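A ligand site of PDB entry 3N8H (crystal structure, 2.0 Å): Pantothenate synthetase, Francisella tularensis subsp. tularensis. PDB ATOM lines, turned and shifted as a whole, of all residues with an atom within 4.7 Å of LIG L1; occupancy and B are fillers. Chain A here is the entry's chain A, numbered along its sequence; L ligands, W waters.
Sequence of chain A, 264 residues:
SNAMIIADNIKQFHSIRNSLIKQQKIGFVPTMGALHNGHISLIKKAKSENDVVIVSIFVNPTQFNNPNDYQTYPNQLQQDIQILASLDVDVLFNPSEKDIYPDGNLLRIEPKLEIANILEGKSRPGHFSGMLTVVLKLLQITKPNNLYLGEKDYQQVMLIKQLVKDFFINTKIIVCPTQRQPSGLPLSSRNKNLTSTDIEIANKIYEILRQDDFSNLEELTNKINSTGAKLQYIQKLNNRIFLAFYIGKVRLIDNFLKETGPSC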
ATOM      1  N   PRO A  30     -11.957 -16.355  -9.651  1.00  0.00           N
ATOM      2  CA  PRO A  30     -12.077 -15.088  -8.899  1.00  0.00           C
ATOM      3  C   PRO A  30     -10.790 -14.278  -9.014  1.00  0.00           C
ATOM      4  O   PRO A  30      -9.703 -14.848  -9.024  1.00  0.00           O
ATOM      5  CB  PRO A  30     -12.287 -15.557  -7.442  1.00  0.00           C
ATOM      6  CG  PRO A  30     -11.575 -16.912  -7.380  1.00  0.00           C
ATOM      7  CD  PRO A  30     -11.765 -17.521  -8.771  1.00  0.00           C
ATOM      8  N   THR A  31     -10.898 -12.953  -9.106  1.00  0.00           N
ATOM      9  CA  THR A  31      -9.694 -12.105  -9.175  1.00  0.00           C
ATOM     10  C   THR A  31     -10.047 -10.776  -8.524  1.00  0.00           C
ATOM     11  O   THR A  31     -11.196 -10.533  -8.192  1.00  0.00           O
ATOM     12  CB  THR A  31      -9.232 -11.844 -10.655  1.00  0.00           C
ATOM     13  OG1 THR A  31      -9.934 -10.726 -11.218  1.00  0.00           O
ATOM     14  CG2 THR A  31      -9.479 -13.061 -11.562  1.00  0.00           C
ATOM     15  N   MET A  32      -9.047  -9.911  -8.371  1.00  0.00           N
ATOM     16  CA  MET A  32      -9.274  -8.549  -7.892  1.00  0.00           C
ATOM     17  C   MET A  32      -8.928  -7.563  -9.019  1.00  0.00           C
ATOM     18  O   MET A  32      -8.565  -6.417  -8.770  1.00  0.00           O
ATOM     19  CB  MET A  32      -8.483  -8.262  -6.619  1.00  0.00           C
ATOM     20  CG  MET A  32      -8.620  -9.353  -5.526  1.00  0.00           C
ATOM     21  SD  MET A  32      -8.357  -8.663  -3.711  1.00  0.00           S
ATOM     22  CE  MET A  32      -6.490  -8.111  -3.889  1.00  0.00           C
ATOM     23  N   GLY A  33      -9.048  -7.999 -10.270  1.00  0.00           N
ATOM     24  CA  GLY A  33      -8.911  -7.091 -11.393  1.00  0.00           C
ATOM     25  C   GLY A  33      -7.457  -6.823 -11.753  1.00  0.00           C
ATOM     26  O   GLY A  33      -6.564  -7.503 -11.235  1.00  0.00           O
ATOM     27  N   HIS A  36      -3.342  -9.818 -15.411  1.00  0.00           N
ATOM     28  CA  HIS A  36      -2.086 -10.099 -16.069  1.00  0.00           C
ATOM     29  C   HIS A  36      -2.055 -11.551 -16.576  1.00  0.00           C
ATOM     30  O   HIS A  36      -3.026 -12.323 -16.435  1.00  0.00           O
ATOM     31  CB  HIS A  36      -0.953  -9.828 -15.106  1.00  0.00           C
ATOM     32  CG  HIS A  36      -1.106 -10.510 -13.788  1.00  0.00           C
ATOM     33  ND1 HIS A  36      -1.058 -11.886 -13.658  1.00  0.00           N
ATOM     34  CD2 HIS A  36      -1.328 -10.020 -12.542  1.00  0.00           C
ATOM     35  CE1 HIS A  36      -1.234 -12.212 -12.389  1.00  0.00           C
ATOM     36  NE2 HIS A  36      -1.392 -11.092 -11.680  1.00  0.00           N
ATOM     37  N   GLY A  38      -0.701 -14.046 -15.454  1.00  0.00           N
ATOM     38  CA  GLY A  38      -1.022 -14.969 -14.385  1.00  0.00           C
ATOM     39  C   GLY A  38      -2.510 -15.290 -14.436  1.00  0.00           C
ATOM     40  O   GLY A  38      -2.915 -16.445 -14.597  1.00  0.00           O
ATOM     41  N   HIS A  39      -3.331 -14.248 -14.330  1.00  0.00           N
ATOM     42  CA  HIS A  39      -4.775 -14.460 -14.407  1.00  0.00           C
ATOM     43  C   HIS A  39      -5.160 -15.120 -15.725  1.00  0.00           C
ATOM     44  O   HIS A  39      -6.069 -15.967 -15.782  1.00  0.00           O
ATOM     45  CB  HIS A  39      -5.525 -13.140 -14.309  1.00  0.00           C
ATOM     46  CG  HIS A  39      -5.262 -12.384 -13.044  1.00  0.00           C
ATOM     47  ND1 HIS A  39      -4.636 -11.155 -13.037  1.00  0.00           N
ATOM     48  CD2 HIS A  39      -5.568 -12.661 -11.750  1.00  0.00           C
ATOM     49  CE1 HIS A  39      -4.566 -10.712 -11.791  1.00  0.00           C
ATOM     50  NE2 HIS A  39      -5.125 -11.604 -10.989  1.00  0.00           N
ATOM     51  N   SER A  41      -3.680 -17.224 -17.549  1.00  0.00           N
ATOM     52  CA  SER A  41      -3.414 -18.657 -17.661  1.00  0.00           C
ATOM     53  C   SER A  41      -4.527 -19.404 -16.980  1.00  0.00           C
ATOM     54  O   SER A  41      -4.962 -20.455 -17.449  1.00  0.00           O
ATOM     55  CB  SER A  41      -2.043 -19.039 -17.094  1.00  0.00           C
ATOM     56  OG  SER A  41      -1.988 -18.760 -15.718  1.00  0.00           O
ATOM     57  N   LEU A  42      -4.999 -18.870 -15.854  1.00  0.00           N
ATOM     58  CA  LEU A  42      -6.116 -19.515 -15.159  1.00  0.00           C
ATOM     59  C   LEU A  42      -7.371 -19.514 -16.050  1.00  0.00           C
ATOM     60  O   LEU A  42      -8.085 -20.527 -16.158  1.00  0.00           O
ATOM     61  CB  LEU A  42      -6.419 -18.850 -13.819  1.00  0.00           C
ATOM     62  CG  LEU A  42      -5.644 -19.313 -12.569  1.00  0.00           C
ATOM     63  CD1 LEU A  42      -4.142 -19.307 -12.779  1.00  0.00           C
ATOM     64  CD2 LEU A  42      -6.003 -18.461 -11.380  1.00  0.00           C
ATOM     65  N   TYR A  73      -4.223   0.071  -4.669  1.00  0.00           N
ATOM     66  CA  TYR A  73      -4.329  -1.192  -5.400  1.00  0.00           C
ATOM     67  C   TYR A  73      -4.706  -0.932  -6.862  1.00  0.00           C
ATOM     68  O   TYR A  73      -5.567  -0.094  -7.141  1.00  0.00           O
ATOM     69  CB  TYR A  73      -5.349  -2.132  -4.749  1.00  0.00           C
ATOM     70  CG  TYR A  73      -5.170  -3.536  -5.307  1.00  0.00           C
ATOM     71  CD1 TYR A  73      -4.147  -4.352  -4.842  1.00  0.00           C
ATOM     72  CD2 TYR A  73      -5.979  -4.007  -6.335  1.00  0.00           C
ATOM     73  CE1 TYR A  73      -3.958  -5.630  -5.353  1.00  0.00           C
ATOM     74  CE2 TYR A  73      -5.801  -5.283  -6.865  1.00  0.00           C
ATOM     75  CZ  TYR A  73      -4.778  -6.095  -6.364  1.00  0.00           C
ATOM     76  OH  TYR A  73      -4.603  -7.365  -6.881  1.00  0.00           O
ATOM     77  N   TYR A 148     -10.623 -22.243 -10.134  1.00  0.00           N
ATOM     78  CA  TYR A 148      -9.215 -22.142 -10.562  1.00  0.00           C
ATOM     79  C   TYR A 148      -8.444 -21.147  -9.703  1.00  0.00           C
ATOM     80  O   TYR A 148      -8.856 -19.988  -9.568  1.00  0.00           O
ATOM     81  CB  TYR A 148      -9.133 -21.821 -12.087  1.00  0.00           C
ATOM     82  CG  TYR A 148      -9.798 -22.926 -12.874  1.00  0.00           C
ATOM     83  CD1 TYR A 148      -9.065 -23.971 -13.397  1.00  0.00           C
ATOM     84  CD2 TYR A 148     -11.170 -22.970 -12.993  1.00  0.00           C
ATOM     85  CE1 TYR A 148      -9.684 -25.043 -14.049  1.00  0.00           C
ATOM     86  CE2 TYR A 148     -11.791 -24.009 -13.642  1.00  0.00           C
ATOM     87  CZ  TYR A 148     -11.054 -25.042 -14.161  1.00  0.00           C
ATOM     88  OH  TYR A 148     -11.725 -26.074 -14.816  1.00  0.00           O
ATOM     89  N   LEU A 149      -7.352 -21.629  -9.099  1.00  0.00           N
ATOM     90  CA  LEU A 149      -6.540 -20.866  -8.151  1.00  0.00           C
ATOM     91  C   LEU A 149      -5.067 -20.998  -8.546  1.00  0.00           C
ATOM     92  O   LEU A 149      -4.648 -22.042  -9.047  1.00  0.00           O
ATOM     93  CB  LEU A 149      -6.727 -21.386  -6.717  1.00  0.00           C
ATOM     94  CG  LEU A 149      -8.107 -21.370  -6.044  1.00  0.00           C
ATOM     95  CD1 LEU A 149      -8.027 -21.976  -4.654  1.00  0.00           C
ATOM     96  CD2 LEU A 149      -8.648 -19.934  -5.964  1.00  0.00           C
ATOM     97  N   GLY A 150      -4.287 -19.939  -8.296  1.00  0.00           N
ATOM     98  CA  GLY A 150      -2.869 -19.967  -8.587  1.00  0.00           C
ATOM     99  C   GLY A 150      -2.084 -20.518  -7.401  1.00  0.00           C
ATOM    100  O   GLY A 150      -2.340 -20.211  -6.237  1.00  0.00           O
ATOM    101  N   LYS A 152       0.777 -19.672  -6.575  1.00  0.00           N
ATOM    102  CA  LYS A 152       1.567 -18.609  -5.955  1.00  0.00           C
ATOM    103  C   LYS A 152       1.058 -18.213  -4.576  1.00  0.00           C
ATOM    104  O   LYS A 152       1.831 -17.891  -3.682  1.00  0.00           O
ATOM    105  CB  LYS A 152       1.585 -17.364  -6.839  1.00  0.00           C
ATOM    106  CG  LYS A 152       2.649 -16.358  -6.412  1.00  0.00           C
ATOM    107  CD  LYS A 152       2.546 -15.077  -7.195  1.00  0.00           C
ATOM    108  CE  LYS A 152       1.610 -14.137  -6.518  1.00  0.00           C
ATOM    109  NZ  LYS A 152       1.091 -13.156  -7.499  1.00  0.00           N
ATOM    110  N   ASP A 153      -0.271 -18.194  -4.425  1.00  0.00           N
ATOM    111  CA  ASP A 153      -0.877 -17.901  -3.141  1.00  0.00           C
ATOM    112  C   ASP A 153      -1.155 -19.241  -2.458  1.00  0.00           C
ATOM    113  O   ASP A 153      -2.309 -19.715  -2.368  1.00  0.00           O
ATOM    114  CB  ASP A 153      -2.123 -17.068  -3.356  1.00  0.00           C
ATOM    115  CG  ASP A 153      -1.809 -15.760  -4.066  1.00  0.00           C
ATOM    116  OD1 ASP A 153      -1.313 -14.838  -3.380  1.00  0.00           O
ATOM    117  OD2 ASP A 153      -2.067 -15.652  -5.292  1.00  0.00           O
ATOM    118  N   GLN A 156      -3.453 -19.533   0.732  1.00  0.00           N
ATOM    119  CA  GLN A 156      -4.777 -19.286   0.172  1.00  0.00           C
ATOM    120  C   GLN A 156      -5.396 -20.566  -0.408  1.00  0.00           C
ATOM    121  O   GLN A 156      -6.551 -20.901  -0.125  1.00  0.00           O
ATOM    122  CB  GLN A 156      -4.692 -18.224  -0.936  1.00  0.00           C
ATOM    123  CG  GLN A 156      -6.032 -17.980  -1.614  1.00  0.00           C
ATOM    124  CD  GLN A 156      -6.079 -16.668  -2.321  1.00  0.00           C
ATOM    125  OE1 GLN A 156      -6.321 -15.622  -1.715  1.00  0.00           O
ATOM    126  NE2 GLN A 156      -5.837 -16.697  -3.625  1.00  0.00           N
ATOM    127  N   CYS A 176      -3.046 -23.997 -10.302  1.00  0.00           N
ATOM    128  CA  CYS A 176      -2.348 -23.691 -11.544  1.00  0.00           C
ATOM    129  C   CYS A 176      -0.976 -23.079 -11.289  1.00  0.00           C
ATOM    130  O   CYS A 176      -0.816 -22.315 -10.356  1.00  0.00           O
ATOM    131  CB  CYS A 176      -3.199 -22.716 -12.382  1.00  0.00           C
ATOM    132  SG  CYS A 176      -4.860 -23.375 -12.823  1.00  0.00           S
ATOM    133  N   PRO A 177       0.011 -23.397 -12.164  1.00  0.00           N
ATOM    134  CA  PRO A 177       1.416 -23.054 -11.968  1.00  0.00           C
ATOM    135  C   PRO A 177       1.601 -21.552 -12.007  1.00  0.00           C
ATOM    136  O   PRO A 177       0.908 -20.847 -12.749  1.00  0.00           O
ATOM    137  CB  PRO A 177       2.114 -23.650 -13.210  1.00  0.00           C
ATOM    138  CG  PRO A 177       1.152 -24.539 -13.839  1.00  0.00           C
ATOM    139  CD  PRO A 177      -0.226 -24.085 -13.449  1.00  0.00           C
ATOM    140  N   THR A 178       2.544 -21.066 -11.227  1.00  0.00           N
ATOM    141  CA  THR A 178       2.838 -19.634 -11.149  1.00  0.00           C
ATOM    142  C   THR A 178       3.508 -19.146 -12.443  1.00  0.00           C
ATOM    143  O   THR A 178       4.559 -19.663 -12.866  1.00  0.00           O
ATOM    144  CB  THR A 178       3.734 -19.348  -9.939  1.00  0.00           C
ATOM    145  OG1 THR A 178       2.999 -19.629  -8.745  1.00  0.00           O
ATOM    146  CG2 THR A 178       4.162 -17.859  -9.917  1.00  0.00           C
ATOM    147  N   GLN A 179       2.890 -18.166 -13.090  1.00  0.00           N
ATOM    148  CA  GLN A 179       3.469 -17.575 -14.280  1.00  0.00           C
ATOM    149  C   GLN A 179       4.513 -16.546 -13.873  1.00  0.00           C
ATOM    150  O   GLN A 179       4.283 -15.753 -12.952  1.00  0.00           O
ATOM    151  CB  GLN A 179       2.383 -16.916 -15.144  1.00  0.00           C
ATOM    152  CG  GLN A 179       1.306 -17.881 -15.605  1.00  0.00           C
ATOM    153  CD  GLN A 179       1.887 -19.094 -16.301  1.00  0.00           C
ATOM    154  OE1 GLN A 179       2.420 -18.991 -17.391  1.00  0.00           O
ATOM    155  NE2 GLN A 179       1.842 -20.246 -15.644  1.00  0.00           N
ATOM    156  N   PRO A 186       7.535 -13.559 -10.255  1.00  0.00           N
ATOM    157  CA  PRO A 186       6.130 -13.893 -10.454  1.00  0.00           C
ATOM    158  C   PRO A 186       5.358 -12.703 -11.020  1.00  0.00           C
ATOM    159  O   PRO A 186       5.587 -11.555 -10.621  1.00  0.00           O
ATOM    160  CB  PRO A 186       5.609 -14.161  -9.045  1.00  0.00           C
ATOM    161  CG  PRO A 186       6.786 -14.432  -8.235  1.00  0.00           C
ATOM    162  CD  PRO A 186       7.939 -13.710  -8.845  1.00  0.00           C
ATOM    163  N   LEU A 187       4.448 -12.973 -11.938  1.00  0.00           N
ATOM    164  CA  LEU A 187       3.490 -11.939 -12.343  1.00  0.00           C
ATOM    165  C   LEU A 187       2.529 -11.636 -11.179  1.00  0.00           C
ATOM    166  O   LEU A 187       2.053 -12.547 -10.485  1.00  0.00           O
ATOM    167  CB  LEU A 187       2.743 -12.375 -13.588  1.00  0.00           C
ATOM    168  CG  LEU A 187       3.707 -12.540 -14.758  1.00  0.00           C
ATOM    169  CD1 LEU A 187       3.001 -13.200 -15.917  1.00  0.00           C
ATOM    170  CD2 LEU A 187       4.285 -11.172 -15.137  1.00  0.00           C
HETATM  171  P1  LIG L   1      -5.377 -11.819  -7.250  1.00  0.00           P
HETATM  172  O1  LIG L   1      -6.155 -11.105  -8.351  1.00  0.00           O
HETATM  173  O2  LIG L   1      -3.928 -11.462  -7.105  1.00  0.00           O
HETATM  174  O3  LIG L   1      -6.095 -11.845  -5.951  1.00  0.00           O
HETATM  175  O4  LIG L   1      -5.247 -13.325  -7.847  1.00  0.00           O
HETATM  176  C1  LIG L   1      -6.358 -14.023  -8.418  1.00  0.00           C
HETATM  177  C2  LIG L   1      -5.968 -15.450  -8.716  1.00  0.00           C
HETATM  178  O5  LIG L   1      -4.871 -15.448  -9.684  1.00  0.00           O
HETATM  179  C3  LIG L   1      -5.483 -16.252  -7.494  1.00  0.00           C
HETATM  180  O6  LIG L   1      -5.868 -17.620  -7.623  1.00  0.00           O
HETATM  181  C4  LIG L   1      -3.961 -16.128  -7.622  1.00  0.00           C
HETATM  182  O7  LIG L   1      -3.204 -17.114  -6.945  1.00  0.00           O
HETATM  183  C5  LIG L   1      -3.784 -16.185  -9.130  1.00  0.00           C
HETATM  184  N1  LIG L   1      -2.492 -15.641  -9.573  1.00  0.00           N
HETATM  185  C6  LIG L   1      -1.978 -14.442  -9.222  1.00  0.00           C
HETATM  186  N2  LIG L   1      -0.743 -14.274  -9.772  1.00  0.00           N
HETATM  187  C7  LIG L   1      -0.443 -15.406 -10.464  1.00  0.00           C
HETATM  188  C8  LIG L   1       0.697 -15.886 -11.268  1.00  0.00           C
HETATM  189  N3  LIG L   1       1.776 -15.104 -11.415  1.00  0.00           N
HETATM  190  N4  LIG L   1       0.632 -17.107 -11.837  1.00  0.00           N
HETATM  191  C9  LIG L   1      -0.462 -17.882 -11.642  1.00  0.00           C
HETATM  192  N5  LIG L   1      -1.542 -17.511 -10.930  1.00  0.00           N
HETATM  193  C10 LIG L   1      -1.597 -16.299 -10.321  1.00  0.00           C
HETATM  194  N1  LG2 L   2      -4.037 -11.401  -3.767  1.00  0.00           N
HETATM  195  C1  LG2 L   2      -4.914 -11.192  -2.628  1.00  0.00           C
HETATM  196  C2  LG2 L   2      -4.496  -9.931  -1.866  1.00  0.00           C
HETATM  197  O1  LG2 L   2      -3.445  -9.360  -2.168  1.00  0.00           O
HETATM  198  C3  LG2 L   2      -4.665 -12.445  -1.781  1.00  0.00           C
HETATM  199  C4  LG2 L   2      -4.328 -13.492  -2.783  1.00  0.00           C
HETATM  200  C5  LG2 L   2      -3.572 -12.799  -3.884  1.00  0.00           C
HETATM  201  O   HOH W   1      -1.658 -12.762  -6.190  1.00  0.00           O
HETATM  202  O   HOH W   2      -5.721  -8.486  -8.870  1.00  0.00           O
HETATM  203  O   HOH W   3      -4.770 -18.868  -5.182  1.00  0.00           O
HETATM  204  O   HOH W   4      -2.985  -9.328  -5.895  1.00  0.00           O
HETATM  205  O   HOH W   5      -8.462 -17.561  -8.620  1.00  0.00           O
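The side-chain carboxylate of Asp 153 is in hydrogen-bond range of an oxygen (O7) of LIG L1 (2.5 Å). O of Leu 187 is in hydrogen-bond range of N3 of LIG L1 (2.7 Å). A nitrogen (N4) of LIG L1 lies within hydrogen-bond range of the backbone NH of Gln 179. The backbone carbonyl oxygen of Gln 179 is in hydrogen-bond range of a nitrogen (N3) of LIG L1. A ring nitrogen (NE2) of His 39 lies within hydrogen-bond range of an oxygen (O1) of LIG L1. N of Gly 150 is in hydrogen-bond range of O6 of LIG L1 (2.9 Å). An oxygen (O7) of LIG L1 is in hydrogen-bond range of the backbone carbonyl oxygen (O) of Gly 150 (3.3 Å). NZ of Lys 152 sits at hydrogen-bond distance from N2 of LIG L1 (3.1 Å). An oxygen (O1) of LIG L1 lies within hydrogen-bond range of the backbone NH (N) of Met 32, 3.1 Å away.
O3 of LIG L1 is in hydrogen-bond range of N1 of LG2 L2, 3.0 Å away.
The backbone carbonyl oxygen (O) of Gln 179 lies within hydrogen-bond range of the backbone NH (N) of Leu 187 (3.0 Å). The backbone carbonyl oxygen of Leu 187 lies within hydrogen-bond range of the side-chain amino group of Lys 152 (3.2 Å). A ring nitrogen (ND1) of His 39 is in hydrogen-bond range of the backbone NH (N) of His 36 (3.0 Å). N of Lys 152 is in hydrogen-bond range of OG1 of Thr 178 (3.1 Å). N of Cys 176 lies within hydrogen-bond range of O of Leu 149, 2.8 Å away. The backbone NH of Gly 38 sits at hydrogen-bond distance from a ring nitrogen (ND1) of His 36. The backbone carbonyl oxygen (O) of Gly 38 sits at hydrogen-bond distance from the side-chain hydroxyl (OG) of Ser 41 (2.7 Å). OG1 of Thr 31 sits at hydrogen-bond distance from N of Gly 33 (3.0 Å).
Merely in contact with LIG L1: Leu 149 (3.4 Å), His 36 (3.4 Å), Thr 178 (3.4 Å), Pro 177 (3.4 Å), Pro 30 (3.5 Å), Leu 42 (3.6 Å), Gly 38 (3.7 Å), Thr 31 (3.8 Å) and Gln 156 (3.9 Å). Hydrophobic or aromatic side chains within 4 Å of LIG L1: Met 32, His 36, His 39, Leu 42, Leu 149 and Leu 187. Within 4 Å of LIG L1: Pro 30, Thr 31, Met 32, His 36, Gly 38, His 39, Leu 42, Leu 149, Gly 150, Lys 152, Asp 153, Gln 156, Pro 177, Thr 178, Gln 179 and Leu 187.
Water W4 lies within hydrogen-bond range of O2 of LIG L1 (2.6 Å), OH of Tyr 73 (2.7 Å) and N1 of LG2 L2 (3.2 Å). Water W2 lies within hydrogen-bond range of the side-chain hydroxyl (OH) of Tyr 73 (2.5 Å), the backbone carbonyl oxygen (O) of Gly 33 (2.7 Å) and an oxygen (O1) of LIG L1 (2.7 Å). Water W1 lies within hydrogen-bond range of an oxygen (O2) of LIG L1, the side-chain carboxylate of Asp 153 and the side-chain amino group of Lys 152. Water W5 lies within hydrogen-bond range of the backbone carbonyl oxygen of Tyr 148 (2.6 Å), an oxygen (O6) of LIG L1 (2.8 Å) and the backbone carbonyl oxygen of Pro 30 (3.0 Å). Water W3 lies within hydrogen-bond range of the side-chain amide nitrogen (NE2) of Gln 156, an oxygen (O7) of LIG L1 and the backbone carbonyl oxygen (O) of Gly 150.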
